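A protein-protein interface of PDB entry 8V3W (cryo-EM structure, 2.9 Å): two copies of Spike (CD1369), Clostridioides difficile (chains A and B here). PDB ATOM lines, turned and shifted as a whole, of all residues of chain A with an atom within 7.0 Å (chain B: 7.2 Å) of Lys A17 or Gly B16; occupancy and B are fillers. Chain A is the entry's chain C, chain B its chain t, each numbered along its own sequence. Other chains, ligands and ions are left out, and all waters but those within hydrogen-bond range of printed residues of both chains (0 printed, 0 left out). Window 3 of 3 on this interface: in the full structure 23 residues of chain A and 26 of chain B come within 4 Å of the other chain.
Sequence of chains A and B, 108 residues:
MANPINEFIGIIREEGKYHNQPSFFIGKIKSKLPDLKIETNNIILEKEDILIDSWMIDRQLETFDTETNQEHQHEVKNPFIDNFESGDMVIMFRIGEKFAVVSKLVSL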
ATOM      1  N   ILE A  12      20.489   9.767  -7.512  1.00  0.00           N
ATOM      2  CA  ILE A  12      21.202   8.652  -6.893  1.00  0.00           C
ATOM      3  C   ILE A  12      22.518   9.130  -6.295  1.00  0.00           C
ATOM      4  O   ILE A  12      22.861   8.801  -5.153  1.00  0.00           O
ATOM      5  CB  ILE A  12      21.433   7.523  -7.912  1.00  0.00           C
ATOM      6  CG1 ILE A  12      20.106   6.914  -8.356  1.00  0.00           C
ATOM      7  CG2 ILE A  12      22.328   6.459  -7.323  1.00  0.00           C
ATOM      8  CD1 ILE A  12      20.260   5.855  -9.409  1.00  0.00           C
ATOM      9  N   ARG A  13      23.273   9.921  -7.061  1.00  0.00           N
ATOM     10  CA  ARG A  13      24.562  10.398  -6.576  1.00  0.00           C
ATOM     11  C   ARG A  13      24.402  11.247  -5.320  1.00  0.00           C
ATOM     12  O   ARG A  13      25.225  11.167  -4.403  1.00  0.00           O
ATOM     13  CB  ARG A  13      25.281  11.190  -7.666  1.00  0.00           C
ATOM     14  CG  ARG A  13      25.762  10.354  -8.834  1.00  0.00           C
ATOM     15  CD  ARG A  13      26.145  11.237 -10.002  1.00  0.00           C
ATOM     16  NE  ARG A  13      26.898  10.514 -11.018  1.00  0.00           N
ATOM     17  CZ  ARG A  13      27.436  11.077 -12.090  1.00  0.00           C
ATOM     18  NH1 ARG A  13      27.326  12.375 -12.316  1.00  0.00           N
ATOM     19  NH2 ARG A  13      28.099  10.321 -12.957  1.00  0.00           N
ATOM     20  N   GLU A  14      23.356  12.072  -5.262  1.00  0.00           N
ATOM     21  CA  GLU A  14      23.165  12.919  -4.088  1.00  0.00           C
ATOM     22  C   GLU A  14      22.684  12.120  -2.882  1.00  0.00           C
ATOM     23  O   GLU A  14      23.184  12.316  -1.770  1.00  0.00           O
ATOM     24  CB  GLU A  14      22.189  14.051  -4.403  1.00  0.00           C
ATOM     25  CG  GLU A  14      22.731  15.064  -5.390  1.00  0.00           C
ATOM     26  CD  GLU A  14      23.816  15.945  -4.804  1.00  0.00           C
ATOM     27  OE1 GLU A  14      24.069  15.859  -3.584  1.00  0.00           O
ATOM     28  OE2 GLU A  14      24.419  16.728  -5.568  1.00  0.00           O
ATOM     29  N   GLU A  15      21.712  11.225  -3.069  1.00  0.00           N
ATOM     30  CA  GLU A  15      21.173  10.473  -1.942  1.00  0.00           C
ATOM     31  C   GLU A  15      22.130   9.408  -1.434  1.00  0.00           C
ATOM     32  O   GLU A  15      21.949   8.920  -0.316  1.00  0.00           O
ATOM     33  CB  GLU A  15      19.844   9.815  -2.314  1.00  0.00           C
ATOM     34  CG  GLU A  15      18.679  10.777  -2.446  1.00  0.00           C
ATOM     35  CD  GLU A  15      18.292  11.410  -1.126  1.00  0.00           C
ATOM     36  OE1 GLU A  15      18.550  10.796  -0.072  1.00  0.00           O
ATOM     37  OE2 GLU A  15      17.721  12.520  -1.140  1.00  0.00           O
ATOM     38  N   GLY A  16      23.140   9.032  -2.218  1.00  0.00           N
ATOM     39  CA  GLY A  16      24.112   8.081  -1.717  1.00  0.00           C
ATOM     40  C   GLY A  16      25.021   8.636  -0.642  1.00  0.00           C
ATOM     41  O   GLY A  16      25.766   7.872  -0.024  1.00  0.00           O
ATOM     42  N   LYS A  17      24.996   9.947  -0.422  1.00  0.00           N
ATOM     43  CA  LYS A  17      25.930  10.609   0.477  1.00  0.00           C
ATOM     44  C   LYS A  17      25.297  11.003   1.802  1.00  0.00           C
ATOM     45  O   LYS A  17      25.895  11.771   2.558  1.00  0.00           O
ATOM     46  CB  LYS A  17      26.515  11.847  -0.202  1.00  0.00           C
ATOM     47  CG  LYS A  17      27.801  11.558  -0.933  1.00  0.00           C
ATOM     48  CD  LYS A  17      27.493  10.604  -2.068  1.00  0.00           C
ATOM     49  CE  LYS A  17      28.713  10.117  -2.788  1.00  0.00           C
ATOM     50  NZ  LYS A  17      28.429   9.979  -4.242  1.00  0.00           N
ATOM     51  N   TYR A  18      24.094  10.505   2.086  1.00  0.00           N
ATOM     52  CA  TYR A  18      23.334  10.980   3.236  1.00  0.00           C
ATOM     53  C   TYR A  18      23.975  10.555   4.552  1.00  0.00           C
ATOM     54  O   TYR A  18      24.023  11.340   5.506  1.00  0.00           O
ATOM     55  CB  TYR A  18      21.900  10.463   3.133  1.00  0.00           C
ATOM     56  CG  TYR A  18      20.922  11.134   4.056  1.00  0.00           C
ATOM     57  CD1 TYR A  18      20.517  12.442   3.831  1.00  0.00           C
ATOM     58  CD2 TYR A  18      20.387  10.459   5.140  1.00  0.00           C
ATOM     59  CE1 TYR A  18      19.620  13.061   4.669  1.00  0.00           C
ATOM     60  CE2 TYR A  18      19.487  11.069   5.982  1.00  0.00           C
ATOM     61  CZ  TYR A  18      19.107  12.371   5.742  1.00  0.00           C
ATOM     62  OH  TYR A  18      18.207  12.987   6.579  1.00  0.00           O
ATOM     63  N   HIS A  19      24.486   9.328   4.621  1.00  0.00           N
ATOM     64  CA  HIS A  19      24.970   8.768   5.876  1.00  0.00           C
ATOM     65  C   HIS A  19      26.444   9.058   6.125  1.00  0.00           C
ATOM     66  O   HIS A  19      26.944   8.738   7.207  1.00  0.00           O
ATOM     67  CB  HIS A  19      24.773   7.248   5.891  1.00  0.00           C
ATOM     68  CG  HIS A  19      23.423   6.810   6.366  1.00  0.00           C
ATOM     69  ND1 HIS A  19      22.774   7.398   7.429  1.00  0.00           N
ATOM     70  CD2 HIS A  19      22.594   5.843   5.905  1.00  0.00           C
ATOM     71  CE1 HIS A  19      21.603   6.813   7.603  1.00  0.00           C
ATOM     72  NE2 HIS A  19      21.470   5.865   6.694  1.00  0.00           N
ATOM     73  N   ASN A  20      27.152   9.632   5.156  1.00  0.00           N
ATOM     74  CA  ASN A  20      28.587   9.832   5.293  1.00  0.00           C
ATOM     75  C   ASN A  20      28.906  10.908   6.321  1.00  0.00           C
ATOM     76  O   ASN A  20      28.164  11.877   6.500  1.00  0.00           O
ATOM     77  CB  ASN A  20      29.213  10.201   3.948  1.00  0.00           C
ATOM     78  CG  ASN A  20      29.003   9.139   2.898  1.00  0.00           C
ATOM     79  OD1 ASN A  20      28.384   8.115   3.159  1.00  0.00           O
ATOM     80  ND2 ASN A  20      29.526   9.373   1.702  1.00  0.00           N
ATOM     81  N   GLN A  21      30.039  10.729   6.989  1.00  0.00           N
ATOM     82  CA  GLN A  21      30.538  11.614   8.025  1.00  0.00           C
ATOM     83  C   GLN A  21      31.956  12.035   7.679  1.00  0.00           C
ATOM     84  O   GLN A  21      32.696  11.273   7.049  1.00  0.00           O
ATOM     85  CB  GLN A  21      30.522  10.918   9.393  1.00  0.00           C
ATOM     86  CG  GLN A  21      29.348  11.307  10.273  1.00  0.00           C
ATOM     87  CD  GLN A  21      29.688  12.418  11.248  1.00  0.00           C
ATOM     88  OE1 GLN A  21      30.618  12.295  12.046  1.00  0.00           O
ATOM     89  NE2 GLN A  21      28.941  13.514  11.183  1.00  0.00           N
ATOM     90  N   GLY B  10      23.562  -3.264  -8.489  1.00  0.00           N
ATOM     91  CA  GLY B  10      24.964  -2.965  -8.739  1.00  0.00           C
ATOM     92  C   GLY B  10      25.184  -1.545  -9.221  1.00  0.00           C
ATOM     93  O   GLY B  10      26.158  -0.890  -8.840  1.00  0.00           O
ATOM     94  N   ILE B  11      24.275  -1.048 -10.062  1.00  0.00           N
ATOM     95  CA  ILE B  11      24.363   0.326 -10.547  1.00  0.00           C
ATOM     96  C   ILE B  11      24.223   1.310  -9.394  1.00  0.00           C
ATOM     97  O   ILE B  11      24.945   2.311  -9.323  1.00  0.00           O
ATOM     98  CB  ILE B  11      23.303   0.566 -11.637  1.00  0.00           C
ATOM     99  CG1 ILE B  11      23.778  -0.009 -12.970  1.00  0.00           C
ATOM    100  CG2 ILE B  11      22.986   2.042 -11.771  1.00  0.00           C
ATOM    101  CD1 ILE B  11      22.786   0.148 -14.088  1.00  0.00           C
ATOM    102  N   ILE B  12      23.287   1.052  -8.480  1.00  0.00           N
ATOM    103  CA  ILE B  12      23.137   1.918  -7.311  1.00  0.00           C
ATOM    104  C   ILE B  12      24.411   1.912  -6.478  1.00  0.00           C
ATOM    105  O   ILE B  12      24.908   2.964  -6.059  1.00  0.00           O
ATOM    106  CB  ILE B  12      21.922   1.494  -6.468  1.00  0.00           C
ATOM    107  CG1 ILE B  12      20.624   1.700  -7.243  1.00  0.00           C
ATOM    108  CG2 ILE B  12      21.887   2.264  -5.169  1.00  0.00           C
ATOM    109  CD1 ILE B  12      19.403   1.233  -6.497  1.00  0.00           C
ATOM    110  N   ARG B  13      24.961   0.723  -6.228  1.00  0.00           N
ATOM    111  CA  ARG B  13      26.170   0.631  -5.416  1.00  0.00           C
ATOM    112  C   ARG B  13      27.326   1.386  -6.058  1.00  0.00           C
ATOM    113  O   ARG B  13      28.127   2.015  -5.359  1.00  0.00           O
ATOM    114  CB  ARG B  13      26.549  -0.830  -5.194  1.00  0.00           C
ATOM    115  CG  ARG B  13      25.597  -1.586  -4.296  1.00  0.00           C
ATOM    116  CD  ARG B  13      25.834  -3.074  -4.398  1.00  0.00           C
ATOM    117  NE  ARG B  13      25.165  -3.808  -3.334  1.00  0.00           N
ATOM    118  CZ  ARG B  13      25.293  -5.111  -3.133  1.00  0.00           C
ATOM    119  NH1 ARG B  13      26.061  -5.856  -3.908  1.00  0.00           N
ATOM    120  NH2 ARG B  13      24.632  -5.680  -2.132  1.00  0.00           N
ATOM    121  N   GLU B  14      27.441   1.325  -7.387  1.00  0.00           N
ATOM    122  CA  GLU B  14      28.543   2.008  -8.058  1.00  0.00           C
ATOM    123  C   GLU B  14      28.342   3.519  -8.093  1.00  0.00           C
ATOM    124  O   GLU B  14      29.276   4.276  -7.815  1.00  0.00           O
ATOM    125  CB  GLU B  14      28.724   1.460  -9.471  1.00  0.00           C
ATOM    126  CG  GLU B  14      29.219   0.028  -9.518  1.00  0.00           C
ATOM    127  CD  GLU B  14      30.671  -0.118  -9.110  1.00  0.00           C
ATOM    128  OE1 GLU B  14      31.349   0.911  -8.905  1.00  0.00           O
ATOM    129  OE2 GLU B  14      31.139  -1.270  -8.986  1.00  0.00           O
ATOM    130  N   GLU B  15      27.137   3.982  -8.433  1.00  0.00           N
ATOM    131  CA  GLU B  15      26.903   5.420  -8.527  1.00  0.00           C
ATOM    132  C   GLU B  15      26.852   6.093  -7.167  1.00  0.00           C
ATOM    133  O   GLU B  15      26.966   7.319  -7.097  1.00  0.00           O
ATOM    134  CB  GLU B  15      25.606   5.716  -9.281  1.00  0.00           C
ATOM    135  CG  GLU B  15      25.670   5.463 -10.774  1.00  0.00           C
ATOM    136  CD  GLU B  15      26.605   6.418 -11.487  1.00  0.00           C
ATOM    137  OE1 GLU B  15      26.820   7.537 -10.978  1.00  0.00           O
ATOM    138  OE2 GLU B  15      27.124   6.054 -12.562  1.00  0.00           O
ATOM    139  N   GLY B  16      26.686   5.333  -6.086  1.00  0.00           N
ATOM    140  CA  GLY B  16      26.730   5.947  -4.775  1.00  0.00           C
ATOM    141  C   GLY B  16      28.107   6.410  -4.354  1.00  0.00           C
ATOM    142  O   GLY B  16      28.230   7.110  -3.345  1.00  0.00           O
ATOM    143  N   LYS B  17      29.146   6.019  -5.087  1.00  0.00           N
ATOM    144  CA  LYS B  17      30.523   6.283  -4.693  1.00  0.00           C
ATOM    145  C   LYS B  17      31.159   7.410  -5.491  1.00  0.00           C
ATOM    146  O   LYS B  17      32.379   7.584  -5.434  1.00  0.00           O
ATOM    147  CB  LYS B  17      31.356   5.009  -4.838  1.00  0.00           C
ATOM    148  CG  LYS B  17      31.399   4.201  -3.566  1.00  0.00           C
ATOM    149  CD  LYS B  17      29.993   3.722  -3.269  1.00  0.00           C
ATOM    150  CE  LYS B  17      29.859   3.030  -1.948  1.00  0.00           C
ATOM    151  NZ  LYS B  17      28.889   1.906  -2.049  1.00  0.00           N
ATOM    152  N   TYR B  18      30.359   8.166  -6.240  1.00  0.00           N
ATOM    153  CA  TYR B  18      30.902   9.137  -7.182  1.00  0.00           C
ATOM    154  C   TYR B  18      31.565  10.309  -6.466  1.00  0.00           C
ATOM    155  O   TYR B  18      32.629  10.777  -6.885  1.00  0.00           O
ATOM    156  CB  TYR B  18      29.784   9.622  -8.102  1.00  0.00           C
ATOM    157  CG  TYR B  18      30.253  10.358  -9.325  1.00  0.00           C
ATOM    158  CD1 TYR B  18      30.881   9.683 -10.360  1.00  0.00           C
ATOM    159  CD2 TYR B  18      30.056  11.723  -9.456  1.00  0.00           C
ATOM    160  CE1 TYR B  18      31.310  10.348 -11.485  1.00  0.00           C
ATOM    161  CE2 TYR B  18      30.481  12.396 -10.577  1.00  0.00           C
ATOM    162  CZ  TYR B  18      31.108  11.703 -11.589  1.00  0.00           C
ATOM    163  OH  TYR B  18      31.534  12.369 -12.713  1.00  0.00           O
ATOM    164  N   HIS B  19      30.963  10.788  -5.380  1.00  0.00           N
ATOM    165  CA  HIS B  19      31.418  12.007  -4.727  1.00  0.00           C
ATOM    166  C   HIS B  19      32.459  11.747  -3.647  1.00  0.00           C
ATOM    167  O   HIS B  19      33.012  12.708  -3.102  1.00  0.00           O
ATOM    168  CB  HIS B  19      30.233  12.742  -4.088  1.00  0.00           C
ATOM    169  CG  HIS B  19      29.511  13.664  -5.017  1.00  0.00           C
ATOM    170  ND1 HIS B  19      30.156  14.473  -5.926  1.00  0.00           N
ATOM    171  CD2 HIS B  19      28.186  13.896  -5.181  1.00  0.00           C
ATOM    172  CE1 HIS B  19      29.261  15.162  -6.611  1.00  0.00           C
ATOM    173  NE2 HIS B  19      28.058  14.833  -6.176  1.00  0.00           N
ATOM    174  N   ASN B  20      32.729  10.487  -3.312  1.00  0.00           N
ATOM    175  CA  ASN B  20      33.635  10.181  -2.214  1.00  0.00           C
ATOM    176  C   ASN B  20      35.077  10.522  -2.565  1.00  0.00           C
ATOM    177  O   ASN B  20      35.505  10.424  -3.717  1.00  0.00           O
ATOM    178  CB  ASN B  20      33.533   8.708  -1.822  1.00  0.00           C
ATOM    179  CG  ASN B  20      32.144   8.317  -1.383  1.00  0.00           C
ATOM    180  OD1 ASN B  20      31.239   9.142  -1.368  1.00  0.00           O
ATOM    181  ND2 ASN B  20      31.967   7.056  -1.019  1.00  0.00           N
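The backbone carbonyl oxygen (O) of Arg A13 sits close to the side-chain amino group (NZ) of Lys A17, 3.4 Å away. The side-chain amino group of Lys B17 sits close to the backbone carbonyl oxygen of Arg B13.
Glu A14 touches none of the printed residues of chain B. Lys A17 touches just these residues of chain B: Gly B16, Lys B17, Tyr B18, His B19 and Asn B20. His A19 touches none of the printed residues of chain B. Printed residues of chain B within 4 Å of Asn A20: Asn B20. Of the printed residues of chain A, Lys B17 touches Lys A17. Printed residues of chain A within 4 Å of His B19: Lys A17 (2.9 Å). The nearest residue of chain B that does not touch Lys A17 is Glu B15 (4.2 Å). The nearest residue of chain A that does not touch Gly B16 is Gly A16 (4.2 Å). The nearest printed residue of chain A that does not touch Glu B15 is Lys A17 (4.2 Å).
NE of Arg A13 lies within salt-bridge range of OE1 of Glu B15 (3.0 Å). The backbone carbonyl oxygen (O) of Gly B16 lies within hydrogen-bond range of the side-chain amino group (NZ) of Lys A17, 3.0 Å away. NZ of Lys A17 sits close to N of Tyr B18, at 3.3 Å. N of His B19 sits close to NZ of Lys A17, at 2.9 Å.
Arg A13 touches Glu B15, but with the chains exchanged Glu A15 does not touch Arg B13 (10.3 Å). Lys A17 touches its own counterpart, Lys B17. Lys A17 touches Tyr B18, but with the chains exchanged Tyr A18 does not touch Lys B17 (9.9 Å). Lys A17 touches His B19, but with the chains exchanged His A19 does not touch Lys B17 (10.3 Å). Of the 9 pairs that touch across the chains among the printed residues, 2 have their exchanged pair printed and touching as well.
Along chain B the printed residues that touch a printed residue of chain A span positions 15 to 20. Of the 10 printed residues of chain A, 4 touch a printed residue of chain B. Hydrophobic or aromatic side chains of chain A that line the printed part of chain B: Ile A12. Among the printed residues, 9 pairs touch across the chains. Among the printed residues, Asp or Glu carboxylates within 4 Å of a Lys or Arg side-chain nitrogen of the other chain: Arg A13 with Glu B15 (3.0 Å).
Ile A12 touches Glu B15 (CG2 to CB, 3.9 Å). NH2 of Arg A13 touches CE1 of Tyr B18, 3.5 Å away. Lys B17 touches Lys A17 (C to NZ, 3.95 Å). Lys A17 touches Asn B20. Asn B20 touches Asn A20.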
